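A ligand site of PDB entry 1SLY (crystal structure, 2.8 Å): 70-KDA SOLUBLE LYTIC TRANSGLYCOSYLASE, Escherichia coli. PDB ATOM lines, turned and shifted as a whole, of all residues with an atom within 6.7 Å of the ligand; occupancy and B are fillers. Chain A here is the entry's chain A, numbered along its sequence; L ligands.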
ATOM      1  N   GLU A 478       3.119 -20.314   9.850  1.00  0.00           N
ATOM      2  CA  GLU A 478       3.493 -19.587   8.641  1.00  0.00           C
ATOM      3  C   GLU A 478       2.325 -18.976   7.891  1.00  0.00           C
ATOM      4  O   GLU A 478       2.319 -17.824   7.516  1.00  0.00           O
ATOM      5  CB  GLU A 478       4.241 -20.508   7.718  1.00  0.00           C
ATOM      6  CG  GLU A 478       5.649 -20.794   8.171  1.00  0.00           C
ATOM      7  CD  GLU A 478       6.690 -19.664   8.036  1.00  0.00           C
ATOM      8  OE1 GLU A 478       6.421 -18.533   7.545  1.00  0.00           O
ATOM      9  OE2 GLU A 478       7.855 -19.914   8.423  1.00  0.00           O
ATOM     10  N   SER A 487       3.492 -13.939   1.072  1.00  0.00           N
ATOM     11  CA  SER A 487       4.122 -12.871   1.880  1.00  0.00           C
ATOM     12  C   SER A 487       4.517 -11.641   1.076  1.00  0.00           C
ATOM     13  O   SER A 487       4.723 -11.753  -0.131  1.00  0.00           O
ATOM     14  CB  SER A 487       5.390 -13.395   2.603  1.00  0.00           C
ATOM     15  OG  SER A 487       6.419 -12.443   2.778  1.00  0.00           O
ATOM     16  N   PRO A 488       4.708 -10.478   1.711  1.00  0.00           N
ATOM     17  CA  PRO A 488       5.266  -9.252   1.105  1.00  0.00           C
ATOM     18  C   PRO A 488       6.419  -9.472   0.141  1.00  0.00           C
ATOM     19  O   PRO A 488       6.397  -9.092  -1.027  1.00  0.00           O
ATOM     20  CB  PRO A 488       5.680  -8.415   2.302  1.00  0.00           C
ATOM     21  CG  PRO A 488       4.488  -8.665   3.128  1.00  0.00           C
ATOM     22  CD  PRO A 488       4.392 -10.165   3.119  1.00  0.00           C
ATOM     23  N   VAL A 489       7.397 -10.174   0.714  1.00  0.00           N
ATOM     24  CA  VAL A 489       8.682 -10.464   0.058  1.00  0.00           C
ATOM     25  C   VAL A 489       8.765 -11.742  -0.811  1.00  0.00           C
ATOM     26  O   VAL A 489       9.849 -12.216  -1.122  1.00  0.00           O
ATOM     27  CB  VAL A 489       9.695 -10.408   1.237  1.00  0.00           C
ATOM     28  CG1 VAL A 489       9.712 -11.675   2.080  1.00  0.00           C
ATOM     29  CG2 VAL A 489      11.016 -10.031   0.635  1.00  0.00           C
ATOM     30  N   GLY A 490       7.648 -12.337  -1.213  1.00  0.00           N
ATOM     31  CA  GLY A 490       7.682 -13.503  -2.086  1.00  0.00           C
ATOM     32  C   GLY A 490       7.430 -14.847  -1.436  1.00  0.00           C
ATOM     33  O   GLY A 490       7.368 -15.827  -2.184  1.00  0.00           O
ATOM     34  N   ALA A 491       7.258 -15.035  -0.128  1.00  0.00           N
ATOM     35  CA  ALA A 491       7.089 -16.407   0.376  1.00  0.00           C
ATOM     36  C   ALA A 491       5.718 -17.023   0.087  1.00  0.00           C
ATOM     37  O   ALA A 491       4.653 -16.464   0.396  1.00  0.00           O
ATOM     38  CB  ALA A 491       7.355 -16.457   1.861  1.00  0.00           C
ATOM     39  N   MET A 495       3.507 -23.557   3.761  1.00  0.00           N
ATOM     40  CA  MET A 495       4.704 -23.447   4.571  1.00  0.00           C
ATOM     41  C   MET A 495       5.563 -22.260   4.180  1.00  0.00           C
ATOM     42  O   MET A 495       6.714 -22.137   4.567  1.00  0.00           O
ATOM     43  CB  MET A 495       5.483 -24.701   4.432  1.00  0.00           C
ATOM     44  CG  MET A 495       4.789 -25.694   5.278  1.00  0.00           C
ATOM     45  SD  MET A 495       5.299 -27.354   4.879  1.00  0.00           S
ATOM     46  CE  MET A 495       6.678 -27.485   6.022  1.00  0.00           C
ATOM     47  N   GLN A 496       5.017 -21.342   3.427  1.00  0.00           N
ATOM     48  CA  GLN A 496       5.701 -20.114   3.071  1.00  0.00           C
ATOM     49  C   GLN A 496       7.141 -20.212   2.642  1.00  0.00           C
ATOM     50  O   GLN A 496       8.028 -19.545   3.149  1.00  0.00           O
ATOM     51  CB  GLN A 496       5.588 -19.145   4.226  1.00  0.00           C
ATOM     52  CG  GLN A 496       4.175 -18.674   4.522  1.00  0.00           C
ATOM     53  CD  GLN A 496       3.699 -17.664   3.518  1.00  0.00           C
ATOM     54  OE1 GLN A 496       4.118 -16.526   3.501  1.00  0.00           O
ATOM     55  NE2 GLN A 496       2.850 -18.031   2.604  1.00  0.00           N
ATOM     56  N   ILE A 497       7.284 -21.019   1.607  1.00  0.00           N
ATOM     57  CA  ILE A 497       8.543 -21.369   0.936  1.00  0.00           C
ATOM     58  C   ILE A 497       8.976 -20.270  -0.007  1.00  0.00           C
ATOM     59  O   ILE A 497       8.190 -19.859  -0.859  1.00  0.00           O
ATOM     60  CB  ILE A 497       8.395 -22.658   0.104  1.00  0.00           C
ATOM     61  CG1 ILE A 497       7.946 -23.778   1.015  1.00  0.00           C
ATOM     62  CG2 ILE A 497       9.711 -23.048  -0.481  1.00  0.00           C
ATOM     63  CD1 ILE A 497       7.338 -25.032   0.455  1.00  0.00           C
ATOM     64  N   MET A 498      10.152 -19.750   0.163  1.00  0.00           N
ATOM     65  CA  MET A 498      10.637 -18.742  -0.762  1.00  0.00           C
ATOM     66  C   MET A 498      10.974 -19.402  -2.115  1.00  0.00           C
ATOM     67  O   MET A 498      11.490 -20.515  -2.131  1.00  0.00           O
ATOM     68  CB  MET A 498      11.890 -18.057  -0.189  1.00  0.00           C
ATOM     69  CG  MET A 498      11.722 -17.183   1.017  1.00  0.00           C
ATOM     70  SD  MET A 498      11.208 -15.501   0.637  1.00  0.00           S
ATOM     71  CE  MET A 498      12.854 -14.981   0.178  1.00  0.00           C
ATOM     72  N   PRO A 499      10.744 -18.772  -3.282  1.00  0.00           N
ATOM     73  CA  PRO A 499      11.123 -19.287  -4.601  1.00  0.00           C
ATOM     74  C   PRO A 499      12.560 -19.785  -4.696  1.00  0.00           C
ATOM     75  O   PRO A 499      12.791 -20.937  -5.079  1.00  0.00           O
ATOM     76  CB  PRO A 499      10.859 -18.130  -5.521  1.00  0.00           C
ATOM     77  CG  PRO A 499       9.684 -17.507  -4.853  1.00  0.00           C
ATOM     78  CD  PRO A 499      10.139 -17.442  -3.441  1.00  0.00           C
ATOM     79  N   GLY A 500      13.496 -18.923  -4.274  1.00  0.00           N
ATOM     80  CA  GLY A 500      14.929 -19.236  -4.259  1.00  0.00           C
ATOM     81  C   GLY A 500      15.235 -20.486  -3.460  1.00  0.00           C
ATOM     82  O   GLY A 500      16.013 -21.329  -3.925  1.00  0.00           O
ATOM     83  N   THR A 501      14.631 -20.664  -2.287  1.00  0.00           N
ATOM     84  CA  THR A 501      14.672 -21.886  -1.456  1.00  0.00           C
ATOM     85  C   THR A 501      14.037 -23.097  -2.123  1.00  0.00           C
ATOM     86  O   THR A 501      14.558 -24.199  -1.946  1.00  0.00           O
ATOM     87  CB  THR A 501      13.943 -21.726  -0.139  1.00  0.00           C
ATOM     88  OG1 THR A 501      14.544 -20.589   0.432  1.00  0.00           O
ATOM     89  CG2 THR A 501      13.946 -22.961   0.762  1.00  0.00           C
ATOM     90  N   ALA A 502      12.921 -22.921  -2.850  1.00  0.00           N
ATOM     91  CA  ALA A 502      12.199 -24.034  -3.528  1.00  0.00           C
ATOM     92  C   ALA A 502      13.087 -24.622  -4.635  1.00  0.00           C
ATOM     93  O   ALA A 502      13.232 -25.823  -4.789  1.00  0.00           O
ATOM     94  CB  ALA A 502      10.898 -23.499  -4.113  1.00  0.00           C
ATOM     95  N   HIS A 504      16.670 -24.305  -4.833  1.00  0.00           N
ATOM     96  CA  HIS A 504      17.746 -25.107  -4.218  1.00  0.00           C
ATOM     97  C   HIS A 504      17.234 -26.419  -3.572  1.00  0.00           C
ATOM     98  O   HIS A 504      17.839 -27.447  -3.798  1.00  0.00           O
ATOM     99  CB  HIS A 504      18.498 -24.308  -3.159  1.00  0.00           C
ATOM    100  CG  HIS A 504      18.877 -22.900  -3.549  1.00  0.00           C
ATOM    101  ND1 HIS A 504      18.613 -21.778  -2.760  1.00  0.00           N
ATOM    102  CD2 HIS A 504      19.507 -22.409  -4.668  1.00  0.00           C
ATOM    103  CE1 HIS A 504      19.056 -20.672  -3.344  1.00  0.00           C
ATOM    104  NE2 HIS A 504      19.590 -21.044  -4.495  1.00  0.00           N
ATOM    105  N   GLY A 530       8.443 -28.180   1.201  1.00  0.00           N
ATOM    106  CA  GLY A 530       8.556 -27.622   2.541  1.00  0.00           C
ATOM    107  C   GLY A 530       9.058 -28.569   3.592  1.00  0.00           C
ATOM    108  O   GLY A 530      10.037 -28.271   4.263  1.00  0.00           O
ATOM    109  N   TYR A 533      12.693 -29.044   2.875  1.00  0.00           N
ATOM    110  CA  TYR A 533      13.542 -28.000   3.498  1.00  0.00           C
ATOM    111  C   TYR A 533      13.607 -28.070   5.047  1.00  0.00           C
ATOM    112  O   TYR A 533      14.661 -27.902   5.656  1.00  0.00           O
ATOM    113  CB  TYR A 533      13.050 -26.618   3.156  1.00  0.00           C
ATOM    114  CG  TYR A 533      14.110 -25.593   3.494  1.00  0.00           C
ATOM    115  CD1 TYR A 533      15.367 -25.695   2.920  1.00  0.00           C
ATOM    116  CD2 TYR A 533      13.844 -24.518   4.345  1.00  0.00           C
ATOM    117  CE1 TYR A 533      16.321 -24.736   3.191  1.00  0.00           C
ATOM    118  CE2 TYR A 533      14.801 -23.556   4.603  1.00  0.00           C
ATOM    119  CZ  TYR A 533      16.034 -23.672   4.019  1.00  0.00           C
ATOM    120  OH  TYR A 533      16.970 -22.706   4.205  1.00  0.00           O
ATOM    121  N   ALA A 551      16.294 -21.494  11.977  1.00  0.00           N
ATOM    122  CA  ALA A 551      16.980 -21.719  10.685  1.00  0.00           C
ATOM    123  C   ALA A 551      15.992 -21.668   9.504  1.00  0.00           C
ATOM    124  O   ALA A 551      16.311 -21.031   8.497  1.00  0.00           O
ATOM    125  CB  ALA A 551      17.678 -23.067  10.681  1.00  0.00           C
ATOM    126  N   TYR A 552      14.811 -22.281   9.578  1.00  0.00           N
ATOM    127  CA  TYR A 552      13.792 -22.185   8.522  1.00  0.00           C
ATOM    128  C   TYR A 552      13.331 -20.733   8.244  1.00  0.00           C
ATOM    129  O   TYR A 552      13.168 -20.334   7.099  1.00  0.00           O
ATOM    130  CB  TYR A 552      12.607 -23.076   8.920  1.00  0.00           C
ATOM    131  CG  TYR A 552      11.547 -23.308   7.862  1.00  0.00           C
ATOM    132  CD1 TYR A 552      10.523 -22.388   7.609  1.00  0.00           C
ATOM    133  CD2 TYR A 552      11.535 -24.494   7.131  1.00  0.00           C
ATOM    134  CE1 TYR A 552       9.531 -22.647   6.674  1.00  0.00           C
ATOM    135  CE2 TYR A 552      10.548 -24.762   6.187  1.00  0.00           C
ATOM    136  CZ  TYR A 552       9.549 -23.842   5.970  1.00  0.00           C
ATOM    137  OH  TYR A 552       8.553 -24.103   5.048  1.00  0.00           O
ATOM    138  N   ASN A 553      13.184 -19.916   9.288  1.00  0.00           N
ATOM    139  CA  ASN A 553      12.794 -18.500   9.169  1.00  0.00           C
ATOM    140  C   ASN A 553      13.873 -17.440   8.806  1.00  0.00           C
ATOM    141  O   ASN A 553      13.598 -16.414   8.157  1.00  0.00           O
ATOM    142  CB  ASN A 553      12.129 -18.108  10.504  1.00  0.00           C
ATOM    143  CG  ASN A 553      11.674 -16.672  10.540  1.00  0.00           C
ATOM    144  OD1 ASN A 553      12.193 -15.816  11.248  1.00  0.00           O
ATOM    145  ND2 ASN A 553      10.732 -16.370   9.694  1.00  0.00           N
ATOM    146  N   ALA A 554      15.071 -17.663   9.329  1.00  0.00           N
ATOM    147  CA  ALA A 554      16.149 -16.708   9.126  1.00  0.00           C
ATOM    148  C   ALA A 554      17.343 -17.233   8.361  1.00  0.00           C
ATOM    149  O   ALA A 554      18.223 -16.506   7.933  1.00  0.00           O
ATOM    150  CB  ALA A 554      16.599 -16.199  10.476  1.00  0.00           C
ATOM    151  N   GLY A 555      17.357 -18.543   8.273  1.00  0.00           N
ATOM    152  CA  GLY A 555      18.398 -19.234   7.568  1.00  0.00           C
ATOM    153  C   GLY A 555      19.485 -19.766   8.477  1.00  0.00           C
ATOM    154  O   GLY A 555      19.925 -19.170   9.457  1.00  0.00           O
ATOM    155  N   LEU A 556      19.846 -20.964   8.129  1.00  0.00           N
ATOM    156  CA  LEU A 556      21.017 -21.672   8.627  1.00  0.00           C
ATOM    157  C   LEU A 556      22.206 -20.906   9.244  1.00  0.00           C
ATOM    158  O   LEU A 556      22.671 -21.118  10.357  1.00  0.00           O
ATOM    159  CB  LEU A 556      21.573 -22.454   7.498  1.00  0.00           C
ATOM    160  CG  LEU A 556      20.693 -23.354   6.688  1.00  0.00           C
ATOM    161  CD1 LEU A 556      19.963 -24.184   7.706  1.00  0.00           C
ATOM    162  CD2 LEU A 556      19.803 -22.587   5.703  1.00  0.00           C
ATOM    163  N   GLY A 557      22.655 -19.971   8.411  1.00  0.00           N
ATOM    164  CA  GLY A 557      23.824 -19.145   8.670  1.00  0.00           C
ATOM    165  C   GLY A 557      23.695 -18.149   9.797  1.00  0.00           C
ATOM    166  O   GLY A 557      24.611 -18.032  10.607  1.00  0.00           O
ATOM    167  N   ARG A 558      22.541 -17.484   9.894  1.00  0.00           N
ATOM    168  CA  ARG A 558      22.262 -16.529  10.958  1.00  0.00           C
ATOM    169  C   ARG A 558      22.197 -17.337  12.230  1.00  0.00           C
ATOM    170  O   ARG A 558      22.782 -16.910  13.230  1.00  0.00           O
ATOM    171  CB  ARG A 558      20.925 -15.824  10.795  1.00  0.00           C
ATOM    172  CG  ARG A 558      21.034 -14.389  11.287  1.00  0.00           C
ATOM    173  CD  ARG A 558      21.391 -13.430  10.174  1.00  0.00           C
ATOM    174  NE  ARG A 558      20.264 -13.382   9.221  1.00  0.00           N
ATOM    175  CZ  ARG A 558      20.170 -12.635   8.105  1.00  0.00           C
ATOM    176  NH1 ARG A 558      21.165 -11.814   7.754  1.00  0.00           N
ATOM    177  NH2 ARG A 558      19.085 -12.704   7.326  1.00  0.00           N
ATOM    178  N   GLU A 583      11.470 -11.039  15.032  1.00  0.00           N
ATOM    179  CA  GLU A 583      10.591 -11.936  14.276  1.00  0.00           C
ATOM    180  C   GLU A 583      10.880 -13.407  14.521  1.00  0.00           C
ATOM    181  O   GLU A 583       9.979 -14.211  14.818  1.00  0.00           O
ATOM    182  CB  GLU A 583      10.723 -11.614  12.799  1.00  0.00           C
ATOM    183  CG  GLU A 583      10.005 -12.452  11.722  1.00  0.00           C
ATOM    184  CD  GLU A 583      10.468 -12.153  10.291  1.00  0.00           C
ATOM    185  OE1 GLU A 583      11.009 -11.048  10.010  1.00  0.00           O
ATOM    186  OE2 GLU A 583      10.290 -13.042   9.433  1.00  0.00           O
ATOM    187  N   TYR A 587       8.883 -16.192  16.524  1.00  0.00           N
ATOM    188  CA  TYR A 587       8.708 -17.403  15.737  1.00  0.00           C
ATOM    189  C   TYR A 587       9.038 -18.688  16.465  1.00  0.00           C
ATOM    190  O   TYR A 587       8.207 -19.602  16.440  1.00  0.00           O
ATOM    191  CB  TYR A 587       9.580 -17.342  14.509  1.00  0.00           C
ATOM    192  CG  TYR A 587       9.316 -18.416  13.466  1.00  0.00           C
ATOM    193  CD1 TYR A 587       9.947 -19.640  13.502  1.00  0.00           C
ATOM    194  CD2 TYR A 587       8.409 -18.170  12.456  1.00  0.00           C
ATOM    195  CE1 TYR A 587       9.692 -20.607  12.550  1.00  0.00           C
ATOM    196  CE2 TYR A 587       8.128 -19.122  11.494  1.00  0.00           C
ATOM    197  CZ  TYR A 587       8.786 -20.328  11.549  1.00  0.00           C
ATOM    198  OH  TYR A 587       8.550 -21.242  10.594  1.00  0.00           O
HETATM  199  C1  LIG L   1      13.431 -17.757   4.827  1.00  0.00           C
HETATM  200  C2  LIG L   1      13.799 -18.944   3.933  1.00  0.00           C
HETATM  201  C3  LIG L   1      15.279 -19.259   4.156  1.00  0.00           C
HETATM  202  C4  LIG L   1      16.145 -17.995   4.021  1.00  0.00           C
HETATM  203  C5  LIG L   1      15.604 -16.828   4.874  1.00  0.00           C
HETATM  204  O1  LIG L   1      14.229 -16.607   4.600  1.00  0.00           O
HETATM  205  O2  LIG L   1      12.109 -17.503   4.560  1.00  0.00           O
HETATM  206  N1  LIG L   1      12.928 -20.087   4.190  1.00  0.00           N
HETATM  207  C6  LIG L   1      12.140 -20.676   3.307  1.00  0.00           C
HETATM  208  O3  LIG L   1      12.093 -20.373   2.119  1.00  0.00           O
HETATM  209  C7  LIG L   1      11.360 -21.858   3.817  1.00  0.00           C
HETATM  210  O4  LIG L   1      15.770 -20.222   3.233  1.00  0.00           O
HETATM  211  O5  LIG L   1      17.444 -18.364   4.470  1.00  0.00           O
HETATM  212  S1  LIG L   1      18.662 -18.399   3.475  1.00  0.00           S
HETATM  213  O6  LIG L   1      18.204 -18.591   2.111  1.00  0.00           O
HETATM  214  O7  LIG L   1      19.504 -19.519   3.832  1.00  0.00           O
HETATM  215  O8  LIG L   1      19.415 -17.169   3.649  1.00  0.00           O
HETATM  216  C8  LIG L   1      16.306 -15.515   4.591  1.00  0.00           C
HETATM  217  O9  LIG L   1      17.130 -15.557   3.436  1.00  0.00           O
HETATM  218  C9  LIG L   1      10.016 -17.227   5.297  1.00  0.00           C
HETATM  219  C10 LIG L   1      11.441 -16.752   5.457  1.00  0.00           C
HETATM  220  C11 LIG L   1      11.300 -15.311   5.059  1.00  0.00           C
HETATM  221  C12 LIG L   1      10.049 -14.929   5.915  1.00  0.00           C
HETATM  222  N2  LIG L   1       9.280 -16.233   6.047  1.00  0.00           N
HETATM  223  C13 LIG L   1       9.776 -18.671   5.705  1.00  0.00           C
HETATM  224  O10 LIG L   1       9.585 -18.568   7.109  1.00  0.00           O
HETATM  225  C14 LIG L   1       9.149 -13.838   5.332  1.00  0.00           C
HETATM  226  O11 LIG L   1       8.598 -13.822   4.227  1.00  0.00           O
HETATM  227  N3  LIG L   1       8.905 -12.953   6.279  1.00  0.00           N
HETATM  228  C15 LIG L   1       8.058 -11.802   6.155  1.00  0.00           C
HETATM  229  C16 LIG L   1       8.872 -10.674   5.556  1.00  0.00           C
HETATM  230  S2  LIG L   1       7.792  -9.232   5.800  1.00  0.00           S
HETATM  231  O12 LIG L   1       8.330  -8.162   4.860  1.00  0.00           O
HETATM  232  O13 LIG L   1       6.344  -9.627   5.574  1.00  0.00           O
HETATM  233  O14 LIG L   1       7.825  -8.798   7.252  1.00  0.00           O
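Merely in contact with the ligand: Pro 488 (3.2 Å), Val 489 (3.2 Å), Ala 491 (3.8 Å), Gln 496 (3.2 Å), Ile 497 (3.8 Å), Asn 553 (3.5 Å), Ala 554 (3.9 Å), Gly 555 (3.4 Å) and Leu 556 (3.6 Å).
Of the 27 residues printed, 16 come within 4 Å of the ligand.
Along chain A the residues within 4 Å of the ligand span positions 478 to 583.
The nearest printed residue that does not touch the ligand is Tyr 587 (4.5 Å).
OE2 of Glu 478 lies within hydrogen-bond range of OH of Tyr 587 (2.6 Å).
The backbone carbonyl oxygen of Met 495 sits at hydrogen-bond distance from the side-chain hydroxyl of Tyr 552, 2.7 Å away.
N of Val 489 is in hydrogen-bond range of OG of Ser 487 (3.2 Å).
The side-chain amide oxygen (OE1) of Gln 496 lies close to the backbone carbonyl oxygen (O) of Ala 491 (3.2 Å).
ND2 of Asn 553 lies within hydrogen-bond range of OE2 of Glu 583 (3.4 Å).
The side-chain carboxylate (OE1) of Glu 478 is in salt-bridge range of a nitrogen (N2) of the ligand (3.96 Å).
N of Met 498 sits at hydrogen-bond distance from O3 of the ligand, 2.8 Å away.
OH of Tyr 533 is in hydrogen-bond range of O4 of the ligand, at 2.9 Å.
A nitrogen (N1) of the ligand is in hydrogen-bond range of the backbone carbonyl oxygen of Tyr 552.
O11 of the ligand is in hydrogen-bond range of OG of Ser 487, at 3.0 Å.
OG1 of Thr 501 lies within hydrogen-bond range of O3 of the ligand (3.0 Å).
OE2 of Glu 583 sits at hydrogen-bond distance from N3 of the ligand (3.4 Å).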
